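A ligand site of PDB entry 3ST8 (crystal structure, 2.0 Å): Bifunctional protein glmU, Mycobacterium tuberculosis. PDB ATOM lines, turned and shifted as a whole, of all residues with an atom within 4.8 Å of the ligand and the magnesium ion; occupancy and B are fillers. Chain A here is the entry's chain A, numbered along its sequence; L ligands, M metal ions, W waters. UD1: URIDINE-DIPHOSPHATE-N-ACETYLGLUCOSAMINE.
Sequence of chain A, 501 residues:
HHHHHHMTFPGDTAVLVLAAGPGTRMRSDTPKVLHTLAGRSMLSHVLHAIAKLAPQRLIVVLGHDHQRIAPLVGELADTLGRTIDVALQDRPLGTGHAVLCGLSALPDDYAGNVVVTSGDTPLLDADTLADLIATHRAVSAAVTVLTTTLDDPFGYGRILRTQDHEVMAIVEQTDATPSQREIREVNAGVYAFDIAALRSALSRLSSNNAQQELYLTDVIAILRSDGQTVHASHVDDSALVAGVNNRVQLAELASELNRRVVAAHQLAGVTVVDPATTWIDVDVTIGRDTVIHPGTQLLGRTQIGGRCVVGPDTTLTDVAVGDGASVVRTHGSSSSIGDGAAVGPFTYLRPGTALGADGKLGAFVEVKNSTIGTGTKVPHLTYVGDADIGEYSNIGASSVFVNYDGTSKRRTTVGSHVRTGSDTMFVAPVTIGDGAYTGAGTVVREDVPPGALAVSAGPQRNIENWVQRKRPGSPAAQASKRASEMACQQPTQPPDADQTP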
ATOM      1  N   LEU A  18     -16.741  16.435  -2.457  1.00  0.00           N
ATOM      2  CA  LEU A  18     -17.539  17.617  -2.810  1.00  0.00           C
ATOM      3  C   LEU A  18     -17.049  18.734  -1.925  1.00  0.00           C
ATOM      4  O   LEU A  18     -17.153  18.645  -0.684  1.00  0.00           O
ATOM      5  CB  LEU A  18     -19.034  17.368  -2.492  1.00  0.00           C
ATOM      6  CG  LEU A  18     -19.610  16.141  -3.201  1.00  0.00           C
ATOM      7  CD1 LEU A  18     -21.150  16.217  -2.920  1.00  0.00           C
ATOM      8  CD2 LEU A  18     -19.311  16.139  -4.788  1.00  0.00           C
ATOM      9  N   ALA A  19     -16.577  19.834  -2.534  1.00  0.00           N
ATOM     10  CA  ALA A  19     -16.028  20.882  -1.696  1.00  0.00           C
ATOM     11  C   ALA A  19     -16.375  22.223  -2.306  1.00  0.00           C
ATOM     12  O   ALA A  19     -15.613  23.166  -2.230  1.00  0.00           O
ATOM     13  CB  ALA A  19     -14.516  20.680  -1.659  1.00  0.00           C
ATOM     14  N   ALA A  20     -17.518  22.281  -2.975  1.00  0.00           N
ATOM     15  CA  ALA A  20     -17.817  23.466  -3.799  1.00  0.00           C
ATOM     16  C   ALA A  20     -18.969  24.264  -3.174  1.00  0.00           C
ATOM     17  O   ALA A  20     -19.409  25.258  -3.744  1.00  0.00           O
ATOM     18  CB  ALA A  20     -18.203  23.044  -5.249  1.00  0.00           C
ATOM     19  N   GLY A  21     -19.489  23.865  -1.984  1.00  0.00           N
ATOM     20  CA  GLY A  21     -20.673  24.627  -1.432  1.00  0.00           C
ATOM     21  C   GLY A  21     -20.132  25.967  -0.839  1.00  0.00           C
ATOM     22  O   GLY A  21     -18.966  26.095  -0.613  1.00  0.00           O
ATOM     23  N   ARG A  25     -22.610  29.060   6.931  1.00  0.00           N
ATOM     24  CA  ARG A  25     -22.781  28.929   8.396  1.00  0.00           C
ATOM     25  C   ARG A  25     -21.392  29.021   9.172  1.00  0.00           C
ATOM     26  O   ARG A  25     -21.343  29.234  10.431  1.00  0.00           O
ATOM     27  CB  ARG A  25     -23.526  27.628   8.685  1.00  0.00           C
ATOM     28  CG  ARG A  25     -25.020  27.820   8.465  1.00  0.00           C
ATOM     29  CD  ARG A  25     -25.683  26.496   8.507  1.00  0.00           C
ATOM     30  NE  ARG A  25     -24.997  25.372   7.806  1.00  0.00           N
ATOM     31  CZ  ARG A  25     -25.442  24.715   6.734  1.00  0.00           C
ATOM     32  NH1 ARG A  25     -26.592  25.063   6.140  1.00  0.00           N
ATOM     33  NH2 ARG A  25     -24.769  23.690   6.233  1.00  0.00           N
ATOM     34  N   LYS A  32     -14.530  27.339   3.821  1.00  0.00           N
ATOM     35  CA  LYS A  32     -14.789  26.380   4.855  1.00  0.00           C
ATOM     36  C   LYS A  32     -13.797  25.186   4.900  1.00  0.00           C
ATOM     37  O   LYS A  32     -13.328  24.772   5.987  1.00  0.00           O
ATOM     38  CB  LYS A  32     -16.206  25.828   4.708  1.00  0.00           C
ATOM     39  CG  LYS A  32     -16.499  24.495   5.555  1.00  0.00           C
ATOM     40  CD  LYS A  32     -17.986  24.148   5.780  1.00  0.00           C
ATOM     41  CE  LYS A  32     -18.567  23.141   4.908  1.00  0.00           C
ATOM     42  NZ  LYS A  32     -19.922  22.816   5.237  1.00  0.00           N
ATOM     43  N   VAL A  61     -14.352  18.482  -6.275  1.00  0.00           N
ATOM     44  CA  VAL A  61     -15.240  19.428  -6.942  1.00  0.00           C
ATOM     45  C   VAL A  61     -15.146  20.736  -6.192  1.00  0.00           C
ATOM     46  O   VAL A  61     -15.460  20.794  -4.973  1.00  0.00           O
ATOM     47  CB  VAL A  61     -16.685  18.899  -6.894  1.00  0.00           C
ATOM     48  CG1 VAL A  61     -17.622  19.875  -7.583  1.00  0.00           C
ATOM     49  CG2 VAL A  61     -16.738  17.473  -7.549  1.00  0.00           C
ATOM     50  N   GLN A  89     -17.782  23.506 -10.259  1.00  0.00           N
ATOM     51  CA  GLN A  89     -19.207  23.600 -10.267  1.00  0.00           C
ATOM     52  C   GLN A  89     -19.422  25.103 -10.205  1.00  0.00           C
ATOM     53  O   GLN A  89     -19.069  25.719  -9.218  1.00  0.00           O
ATOM     54  CB  GLN A  89     -19.805  22.899  -9.017  1.00  0.00           C
ATOM     55  CG  GLN A  89     -21.405  23.103  -8.856  1.00  0.00           C
ATOM     56  CD  GLN A  89     -21.926  22.586  -7.524  1.00  0.00           C
ATOM     57  OE1 GLN A  89     -21.283  22.767  -6.484  1.00  0.00           O
ATOM     58  NE2 GLN A  89     -23.115  22.047  -7.529  1.00  0.00           N
ATOM     59  N   PRO A  92     -23.611  26.731  -6.685  1.00  0.00           N
ATOM     60  CA  PRO A  92     -23.849  25.580  -5.772  1.00  0.00           C
ATOM     61  C   PRO A  92     -25.298  25.093  -5.862  1.00  0.00           C
ATOM     62  O   PRO A  92     -26.115  25.454  -5.001  1.00  0.00           O
ATOM     63  CB  PRO A  92     -23.531  26.167  -4.388  1.00  0.00           C
ATOM     64  CG  PRO A  92     -23.805  27.659  -4.523  1.00  0.00           C
ATOM     65  CD  PRO A  92     -23.533  28.029  -5.985  1.00  0.00           C
ATOM     66  N   LEU A  93     -25.609  24.304  -6.892  1.00  0.00           N
ATOM     67  CA  LEU A  93     -27.024  23.979  -7.202  1.00  0.00           C
ATOM     68  C   LEU A  93     -27.449  22.762  -6.396  1.00  0.00           C
ATOM     69  O   LEU A  93     -28.576  22.282  -6.534  1.00  0.00           O
ATOM     70  CB  LEU A  93     -27.190  23.669  -8.673  1.00  0.00           C
ATOM     71  CG  LEU A  93     -26.997  24.980  -9.499  1.00  0.00           C
ATOM     72  CD1 LEU A  93     -27.299  24.711 -10.993  1.00  0.00           C
ATOM     73  CD2 LEU A  93     -27.851  26.079  -8.913  1.00  0.00           C
ATOM     74  N   GLY A  94     -26.512  22.222  -5.605  1.00  0.00           N
ATOM     75  CA  GLY A  94     -26.895  21.106  -4.701  1.00  0.00           C
ATOM     76  C   GLY A  94     -25.898  19.975  -4.759  1.00  0.00           C
ATOM     77  O   GLY A  94     -25.098  19.879  -5.737  1.00  0.00           O
ATOM     78  N   THR A  95     -25.891  19.116  -3.712  1.00  0.00           N
ATOM     79  CA  THR A  95     -24.909  18.063  -3.712  1.00  0.00           C
ATOM     80  C   THR A  95     -25.046  17.135  -4.916  1.00  0.00           C
ATOM     81  O   THR A  95     -24.033  16.545  -5.403  1.00  0.00           O
ATOM     82  CB  THR A  95     -24.992  17.218  -2.354  1.00  0.00           C
ATOM     83  OG1 THR A  95     -26.343  16.786  -2.160  1.00  0.00           O
ATOM     84  CG2 THR A  95     -24.590  18.110  -1.186  1.00  0.00           C
ATOM     85  N   ALA A  98     -23.357  18.776  -7.731  1.00  0.00           N
ATOM     86  CA  ALA A  98     -21.885  18.705  -7.499  1.00  0.00           C
ATOM     87  C   ALA A  98     -21.360  17.356  -8.010  1.00  0.00           C
ATOM     88  O   ALA A  98     -20.310  17.298  -8.659  1.00  0.00           O
ATOM     89  CB  ALA A  98     -21.596  18.845  -5.928  1.00  0.00           C
ATOM     90  N   SER A 118     -17.668  14.291   1.464  1.00  0.00           N
ATOM     91  CA  SER A 118     -17.591  15.721   1.530  1.00  0.00           C
ATOM     92  C   SER A 118     -16.243  16.167   1.990  1.00  0.00           C
ATOM     93  O   SER A 118     -15.564  15.458   2.681  1.00  0.00           O
ATOM     94  CB  SER A 118     -18.547  16.271   2.594  1.00  0.00           C
ATOM     95  OG  SER A 118     -19.819  15.692   2.320  1.00  0.00           O
ATOM     96  N   GLY A 119     -15.912  17.391   1.658  1.00  0.00           N
ATOM     97  CA  GLY A 119     -14.737  17.947   2.195  1.00  0.00           C
ATOM     98  C   GLY A 119     -14.830  18.381   3.705  1.00  0.00           C
ATOM     99  O   GLY A 119     -13.843  18.872   4.162  1.00  0.00           O
ATOM    100  N   ASP A 120     -16.021  18.342   4.346  1.00  0.00           N
ATOM    101  CA  ASP A 120     -16.189  18.794   5.762  1.00  0.00           C
ATOM    102  C   ASP A 120     -16.403  17.609   6.757  1.00  0.00           C
ATOM    103  O   ASP A 120     -17.139  17.752   7.759  1.00  0.00           O
ATOM    104  CB  ASP A 120     -17.352  19.811   5.839  1.00  0.00           C
ATOM    105  CG  ASP A 120     -18.680  19.226   5.461  1.00  0.00           C
ATOM    106  OD1 ASP A 120     -18.765  18.013   5.075  1.00  0.00           O
ATOM    107  OD2 ASP A 120     -19.695  19.971   5.483  1.00  0.00           O
ATOM    108  N   THR A 121     -15.826  16.421   6.441  1.00  0.00           N
ATOM    109  CA  THR A 121     -15.928  15.204   7.271  1.00  0.00           C
ATOM    110  C   THR A 121     -14.487  14.788   7.577  1.00  0.00           C
ATOM    111  O   THR A 121     -13.993  13.827   6.998  1.00  0.00           O
ATOM    112  CB  THR A 121     -16.785  14.100   6.520  1.00  0.00           C
ATOM    113  OG1 THR A 121     -18.167  14.544   6.396  1.00  0.00           O
ATOM    114  CG2 THR A 121     -16.993  12.776   7.332  1.00  0.00           C
ATOM    115  N   GLY A 155     -29.689  18.947  11.793  1.00  0.00           N
ATOM    116  CA  GLY A 155     -28.808  19.264  10.671  1.00  0.00           C
ATOM    117  C   GLY A 155     -28.502  18.130   9.685  1.00  0.00           C
ATOM    118  O   GLY A 155     -28.288  18.368   8.475  1.00  0.00           O
ATOM    119  N   TYR A 156     -28.556  16.876  10.159  1.00  0.00           N
ATOM    120  CA  TYR A 156     -28.335  15.763   9.228  1.00  0.00           C
ATOM    121  C   TYR A 156     -29.565  15.274   8.426  1.00  0.00           C
ATOM    122  O   TYR A 156     -30.707  15.327   8.911  1.00  0.00           O
ATOM    123  CB  TYR A 156     -27.760  14.594   9.993  1.00  0.00           C
ATOM    124  CG  TYR A 156     -26.307  14.744  10.608  1.00  0.00           C
ATOM    125  CD1 TYR A 156     -25.181  14.122   9.956  1.00  0.00           C
ATOM    126  CD2 TYR A 156     -26.086  15.395  11.837  1.00  0.00           C
ATOM    127  CE1 TYR A 156     -23.837  14.142  10.476  1.00  0.00           C
ATOM    128  CE2 TYR A 156     -24.750  15.473  12.360  1.00  0.00           C
ATOM    129  CZ  TYR A 156     -23.676  14.822  11.662  1.00  0.00           C
ATOM    130  OH  TYR A 156     -22.455  14.897  12.174  1.00  0.00           O
ATOM    131  N   GLY A 157     -29.348  14.655   7.238  1.00  0.00           N
ATOM    132  CA  GLY A 157     -30.455  13.929   6.583  1.00  0.00           C
ATOM    133  C   GLY A 157     -30.867  12.707   7.483  1.00  0.00           C
ATOM    134  O   GLY A 157     -29.999  12.026   8.062  1.00  0.00           O
ATOM    135  N   ILE A 170     -33.640   8.996   2.266  1.00  0.00           N
ATOM    136  CA  ILE A 170     -33.084   9.949   3.232  1.00  0.00           C
ATOM    137  C   ILE A 170     -33.865  11.252   3.130  1.00  0.00           C
ATOM    138  O   ILE A 170     -34.165  11.716   2.006  1.00  0.00           O
ATOM    139  CB  ILE A 170     -31.605  10.235   2.881  1.00  0.00           C
ATOM    140  CG1 ILE A 170     -30.817   8.925   2.963  1.00  0.00           C
ATOM    141  CG2 ILE A 170     -31.012  11.433   3.744  1.00  0.00           C
ATOM    142  CD1 ILE A 170     -29.328   9.069   2.387  1.00  0.00           C
ATOM    143  N   GLU A 172     -34.018  15.323   4.350  1.00  0.00           N
ATOM    144  CA  GLU A 172     -33.104  16.403   4.852  1.00  0.00           C
ATOM    145  C   GLU A 172     -33.753  17.155   6.026  1.00  0.00           C
ATOM    146  O   GLU A 172     -34.965  17.272   6.058  1.00  0.00           O
ATOM    147  CB  GLU A 172     -32.775  17.394   3.701  1.00  0.00           C
ATOM    148  CG  GLU A 172     -31.785  16.788   2.637  1.00  0.00           C
ATOM    149  CD  GLU A 172     -30.538  16.319   3.311  1.00  0.00           C
ATOM    150  OE1 GLU A 172     -29.762  17.177   3.749  1.00  0.00           O
ATOM    151  OE2 GLU A 172     -30.310  15.103   3.454  1.00  0.00           O
ATOM    152  N   ASN A 187     -27.623  10.360   7.877  1.00  0.00           N
ATOM    153  CA  ASN A 187     -26.795  10.147   6.696  1.00  0.00           C
ATOM    154  C   ASN A 187     -25.350  10.770   6.927  1.00  0.00           C
ATOM    155  O   ASN A 187     -25.315  11.962   7.117  1.00  0.00           O
ATOM    156  CB  ASN A 187     -27.447  10.942   5.597  1.00  0.00           C
ATOM    157  CG  ASN A 187     -26.651  10.856   4.256  1.00  0.00           C
ATOM    158  OD1 ASN A 187     -25.885   9.920   4.050  1.00  0.00           O
ATOM    159  ND2 ASN A 187     -26.845  11.853   3.375  1.00  0.00           N
ATOM    160  N   ALA A 188     -24.298   9.984   6.847  1.00  0.00           N
ATOM    161  CA  ALA A 188     -22.913  10.527   6.992  1.00  0.00           C
ATOM    162  C   ALA A 188     -22.544  11.321   5.707  1.00  0.00           C
ATOM    163  O   ALA A 188     -21.551  12.037   5.690  1.00  0.00           O
ATOM    164  CB  ALA A 188     -22.020   9.432   7.149  1.00  0.00           C
ATOM    165  N   GLY A 189     -23.283  11.165   4.613  1.00  0.00           N
ATOM    166  CA  GLY A 189     -22.961  11.935   3.361  1.00  0.00           C
ATOM    167  C   GLY A 189     -21.751  11.276   2.669  1.00  0.00           C
ATOM    168  O   GLY A 189     -20.988  11.965   1.963  1.00  0.00           O
ATOM    169  N   TYR A 191     -20.824   7.809   0.386  1.00  0.00           N
ATOM    170  CA  TYR A 191     -21.637   6.793  -0.380  1.00  0.00           C
ATOM    171  C   TYR A 191     -20.709   6.035  -1.321  1.00  0.00           C
ATOM    172  O   TYR A 191     -19.656   6.607  -1.743  1.00  0.00           O
ATOM    173  CB  TYR A 191     -22.533   7.532  -1.371  1.00  0.00           C
ATOM    174  CG  TYR A 191     -23.389   8.619  -0.806  1.00  0.00           C
ATOM    175  CD1 TYR A 191     -22.871   9.882  -0.559  1.00  0.00           C
ATOM    176  CD2 TYR A 191     -24.747   8.412  -0.526  1.00  0.00           C
ATOM    177  CE1 TYR A 191     -23.649  10.910  -0.083  1.00  0.00           C
ATOM    178  CE2 TYR A 191     -25.589   9.471  -0.051  1.00  0.00           C
ATOM    179  CZ  TYR A 191     -25.019  10.669   0.219  1.00  0.00           C
ATOM    180  OH  TYR A 191     -25.792  11.714   0.588  1.00  0.00           O
ATOM    181  N   TYR A 215     -30.637  17.460  -4.636  1.00  0.00           N
ATOM    182  CA  TYR A 215     -30.094  16.684  -3.485  1.00  0.00           C
ATOM    183  C   TYR A 215     -29.521  15.366  -3.921  1.00  0.00           C
ATOM    184  O   TYR A 215     -30.249  14.454  -4.443  1.00  0.00           O
ATOM    185  CB  TYR A 215     -31.202  16.363  -2.448  1.00  0.00           C
ATOM    186  CG  TYR A 215     -31.868  17.522  -1.684  1.00  0.00           C
ATOM    187  CD1 TYR A 215     -31.249  18.762  -1.540  1.00  0.00           C
ATOM    188  CD2 TYR A 215     -33.147  17.338  -1.042  1.00  0.00           C
ATOM    189  CE1 TYR A 215     -31.850  19.810  -0.763  1.00  0.00           C
ATOM    190  CE2 TYR A 215     -33.754  18.379  -0.280  1.00  0.00           C
ATOM    191  CZ  TYR A 215     -33.110  19.573  -0.152  1.00  0.00           C
ATOM    192  OH  TYR A 215     -33.700  20.566   0.558  1.00  0.00           O
ATOM    193  N   LEU A 216     -28.262  15.138  -3.573  1.00  0.00           N
ATOM    194  CA  LEU A 216     -27.679  13.814  -3.852  1.00  0.00           C
ATOM    195  C   LEU A 216     -28.516  12.769  -3.081  1.00  0.00           C
ATOM    196  O   LEU A 216     -28.632  11.613  -3.530  1.00  0.00           O
ATOM    197  CB  LEU A 216     -26.235  13.744  -3.309  1.00  0.00           C
ATOM    198  CG  LEU A 216     -25.605  12.358  -3.509  1.00  0.00           C
ATOM    199  CD1 LEU A 216     -25.558  12.023  -4.958  1.00  0.00           C
ATOM    200  CD2 LEU A 216     -24.116  12.425  -3.042  1.00  0.00           C
ATOM    201  N   THR A 217     -29.076  13.161  -1.913  1.00  0.00           N
ATOM    202  CA  THR A 217     -29.722  12.175  -0.978  1.00  0.00           C
ATOM    203  C   THR A 217     -30.994  11.587  -1.657  1.00  0.00           C
ATOM    204  O   THR A 217     -31.429  10.503  -1.287  1.00  0.00           O
ATOM    205  CB  THR A 217     -30.054  12.861   0.373  1.00  0.00           C
ATOM    206  OG1 THR A 217     -30.665  14.128   0.061  1.00  0.00           O
ATOM    207  CG2 THR A 217     -28.806  13.141   1.146  1.00  0.00           C
ATOM    208  N   GLY A 243     -19.776  15.674  10.544  1.00  0.00           N
ATOM    209  CA  GLY A 243     -19.451  16.764   9.679  1.00  0.00           C
ATOM    210  C   GLY A 243     -19.370  18.074  10.386  1.00  0.00           C
ATOM    211  O   GLY A 243     -19.831  18.204  11.529  1.00  0.00           O
ATOM    212  N   VAL A 244     -18.775  19.014   9.691  1.00  0.00           N
ATOM    213  CA  VAL A 244     -18.501  20.339  10.159  1.00  0.00           C
ATOM    214  C   VAL A 244     -19.195  21.427   9.246  1.00  0.00           C
ATOM    215  O   VAL A 244     -18.692  21.764   8.114  1.00  0.00           O
ATOM    216  CB  VAL A 244     -17.069  20.568  10.142  1.00  0.00           C
ATOM    217  CG1 VAL A 244     -16.773  21.998  10.513  1.00  0.00           C
ATOM    218  CG2 VAL A 244     -16.372  19.473  11.127  1.00  0.00           C
ATOM    219  N   ASN A 245     -20.322  21.964   9.753  1.00  0.00           N
ATOM    220  CA  ASN A 245     -20.970  23.126   9.032  1.00  0.00           C
ATOM    221  C   ASN A 245     -20.755  24.495   9.712  1.00  0.00           C
ATOM    222  O   ASN A 245     -21.035  25.550   9.104  1.00  0.00           O
ATOM    223  CB  ASN A 245     -22.492  22.811   8.896  1.00  0.00           C
ATOM    224  CG  ASN A 245     -22.776  21.669   7.946  1.00  0.00           C
ATOM    225  OD1 ASN A 245     -21.923  21.375   7.085  1.00  0.00           O
ATOM    226  ND2 ASN A 245     -24.027  20.977   8.065  1.00  0.00           N
HETATM  227  C1' UD1 L   1     -25.259  16.831   3.827  1.00  0.00           C
HETATM  228  C2' UD1 L   1     -26.360  15.881   3.370  1.00  0.00           C
HETATM  229  C3' UD1 L   1     -26.991  15.161   4.547  1.00  0.00           C
HETATM  230  C4' UD1 L   1     -25.920  14.562   5.454  1.00  0.00           C
HETATM  231  C5' UD1 L   1     -24.847  15.584   5.790  1.00  0.00           C
HETATM  232  C6' UD1 L   1     -23.741  14.960   6.638  1.00  0.00           C
HETATM  233  C7' UD1 L   1     -27.444  16.566   1.304  1.00  0.00           C
HETATM  234  C8' UD1 L   1     -28.690  17.139   0.709  1.00  0.00           C
HETATM  235  N2' UD1 L   1     -27.370  16.617   2.639  1.00  0.00           N
HETATM  236  O1' UD1 L   1     -25.821  17.861   4.637  1.00  0.00           O
HETATM  237  O3' UD1 L   1     -27.854  14.127   4.076  1.00  0.00           O
HETATM  238  O4' UD1 L   1     -26.528  14.095   6.668  1.00  0.00           O
HETATM  239  O5' UD1 L   1     -24.292  16.099   4.582  1.00  0.00           O
HETATM  240  O6' UD1 L   1     -22.612  15.839   6.674  1.00  0.00           O
HETATM  241  O7' UD1 L   1     -26.569  16.077   0.628  1.00  0.00           O
HETATM  242  N1  UD1 L   1     -21.406  20.898  -1.924  1.00  0.00           N
HETATM  243  C2  UD1 L   1     -21.153  21.252  -3.258  1.00  0.00           C
HETATM  244  N3  UD1 L   1     -22.093  21.872  -3.983  1.00  0.00           N
HETATM  245  C4  UD1 L   1     -23.283  22.169  -3.447  1.00  0.00           C
HETATM  246  C5  UD1 L   1     -23.549  21.831  -2.122  1.00  0.00           C
HETATM  247  C6  UD1 L   1     -22.588  21.185  -1.372  1.00  0.00           C
HETATM  248  O2  UD1 L   1     -20.044  20.974  -3.782  1.00  0.00           O
HETATM  249  O4  UD1 L   1     -24.150  22.744  -4.133  1.00  0.00           O
HETATM  250  C1B UD1 L   1     -20.371  20.208  -1.136  1.00  0.00           C
HETATM  251  C2B UD1 L   1     -19.919  21.119   0.007  1.00  0.00           C
HETATM  252  O2' UD1 L   1     -18.503  21.341  -0.097  1.00  0.00           O
HETATM  253  C3B UD1 L   1     -20.232  20.369   1.280  1.00  0.00           C
HETATM  254  C4B UD1 L   1     -20.862  19.047   0.870  1.00  0.00           C
HETATM  255  O4B UD1 L   1     -20.917  19.026  -0.558  1.00  0.00           O
HETATM  256  O3B UD1 L   1     -19.014  20.121   1.996  1.00  0.00           O
HETATM  257  C5B UD1 L   1     -22.260  18.903   1.440  1.00  0.00           C
HETATM  258  O5B UD1 L   1     -22.858  20.191   1.549  1.00  0.00           O
HETATM  259  PA  UD1 L   1     -23.477  20.688   2.955  1.00  0.00           P
HETATM  260  O1A UD1 L   1     -24.178  22.011   2.724  1.00  0.00           O
HETATM  261  O2A UD1 L   1     -22.411  20.573   4.011  1.00  0.00           O
HETATM  262  O3A UD1 L   1     -24.606  19.569   3.253  1.00  0.00           O
HETATM  263  PB  UD1 L   1     -25.086  19.293   4.759  1.00  0.00           P
HETATM  264  O1B UD1 L   1     -23.863  19.125   5.628  1.00  0.00           O
HETATM  265  O2B UD1 L   1     -26.129  20.320   5.132  1.00  0.00           O
HETATM  266 MG    MG M   1     -21.765  19.594   5.675  1.00  0.00          MG
HETATM  267  O   HOH W   1     -28.728  19.825   3.523  1.00  0.00           O
HETATM  268  O   HOH W   2     -27.093  22.825   3.106  1.00  0.00           O
HETATM  269  O   HOH W   3     -27.256  20.801   7.379  1.00  0.00           O
HETATM  270  O   HOH W   4     -20.817  14.047   7.756  1.00  0.00           O
HETATM  271  O   HOH W   5     -21.651  18.401   7.535  1.00  0.00           O
HETATM  272  O   HOH W   6     -27.906  20.324   1.082  1.00  0.00           O
HETATM  273  O   HOH W   7     -17.534  24.025   1.469  1.00  0.00           O
HETATM  274  O   HOH W   8     -21.589  17.746   4.804  1.00  0.00           O
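O4' of the ligand is in hydrogen-bond range of O of Asn 187, 2.5 Å away.
ND2 of Asn 187 is in hydrogen-bond range of O3' of the ligand, 2.6 Å away.
OE1 of Glu 172 sits at hydrogen-bond distance from N2' of the ligand, 2.7 Å away.
The side-chain amide oxygen (OE1) of Gln 89 lies within hydrogen-bond range of a nitrogen (N3) of the ligand, 2.8 Å away.
The backbone NH (N) of Gly 94 sits at hydrogen-bond distance from an oxygen (O4) of the ligand, at 2.8 Å.
The side-chain hydroxyl (OG1) of Thr 95 lies within hydrogen-bond range of an oxygen (O7') of the ligand (2.9 Å).
The backbone NH of Gly 157 lies within hydrogen-bond range of an oxygen (O4') of the ligand (2.9 Å).
An oxygen (O2) of the ligand is in hydrogen-bond range of the backbone NH (N) of Ala 20 (3.0 Å).
The backbone NH of Ala 19 lies close to an oxygen (O2') of the ligand (3.5 Å).
The backbone carbonyl oxygen of Leu 18 sits at hydrogen-bond distance from an oxygen (O2') of the ligand, at 3.1 Å.
An oxygen (O2') of the ligand lies within hydrogen-bond range of the backbone NH (N) of Gly 21 (3.3 Å).
N of Leu 93 lies within hydrogen-bond range of O4 of the ligand.
O2A of the ligand sits close to NZ of Lys 32 (3.6 Å).
An oxygen (O2B) of the ligand lies within salt-bridge range of the guanidinium group of Arg 25.
The side-chain amide oxygen (OD1) of Asn 245 lies close to the side-chain amino group (NZ) of Lys 32 (3.1 Å).
The side-chain amide oxygen (OD1) of Asn 187 sits at hydrogen-bond distance from the backbone NH (N) of Gly 189 (2.9 Å).
The side-chain amide nitrogen (ND2) of Asn 187 sits at hydrogen-bond distance from the side-chain hydroxyl (OH) of Tyr 191, 3.0 Å away.
NE2 of Gln 89 sits close to N of Ala 98 (3.3 Å).
N of Leu 93 lies close to NE2 of Gln 89, 3.4 Å away.
N of Ala 20 is in hydrogen-bond range of O of Val 61 (3.2 Å).
The backbone carbonyl oxygen (O) of Leu 18 is in hydrogen-bond range of the backbone NH (N) of Gly 119, at 2.9 Å.
The backbone carbonyl oxygen (O) of Val 244 lies within hydrogen-bond range of the side-chain amino group (NZ) of Lys 32, at 3.3 Å.
O of Pro 92 sits close to O4 of the ligand (3.5 Å).
CB of Ala 98 touches O2 of the ligand (3.4 Å).
Ser 118 touches the ligand (OG to C4B, 3.8 Å).
CA of Tyr 156 touches O4' of the ligand, 3.5 Å away.
Ala 188 touches the ligand (O to C6', 3.8 Å).
CD1 of Tyr 215 touches C8' of the ligand, at 3.8 Å.
Thr 217 touches the ligand (CG2 to O3', 3.2 Å).
The nearest printed residue that does not touch the ligand is Gly 119 (4.1 Å).
NZ of Lys 32 touches the magnesium ion, 3.7 Å away.
Within 4 Å of the magnesium ion: Lys 32, Asp 120 and Asn 245.
The magnesium ion is bound by O2A of the ligand, 2.0 Å away.
Water W8 is bound to the magnesium ion (2.1 Å).
OD2 of Asp 120 is bound to the magnesium ion (2.1 Å).
The magnesium ion is bound by O1B of the ligand (2.2 Å).
Water W5 is bound to the magnesium ion (2.2 Å).
OD1 of Asn 245 binds the magnesium ion.
The magnesium ion has six donor atoms within binding distance.
Water W8 bridges OD1 of Asp 120 (2.8 Å) and O6' of the ligand (2.9 Å).
Water W3 lies within hydrogen-bond range of an oxygen (O2B) of the ligand, the backbone carbonyl oxygen of Gly 155 and the side-chain amide nitrogen of Asn 245.
Water W4 lies within hydrogen-bond range of O6' of the ligand, O of Ala 188, OG1 of Thr 121 and N of Gly 243.
Water W1 bridges OE1 of Glu 172 (2.9 Å) and O2B of the ligand (3.1 Å).
Water W7 bridges an oxygen (O2') of the ligand (3.3 Å) and the backbone carbonyl oxygen (O) of Gly 21 (3.3 Å).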
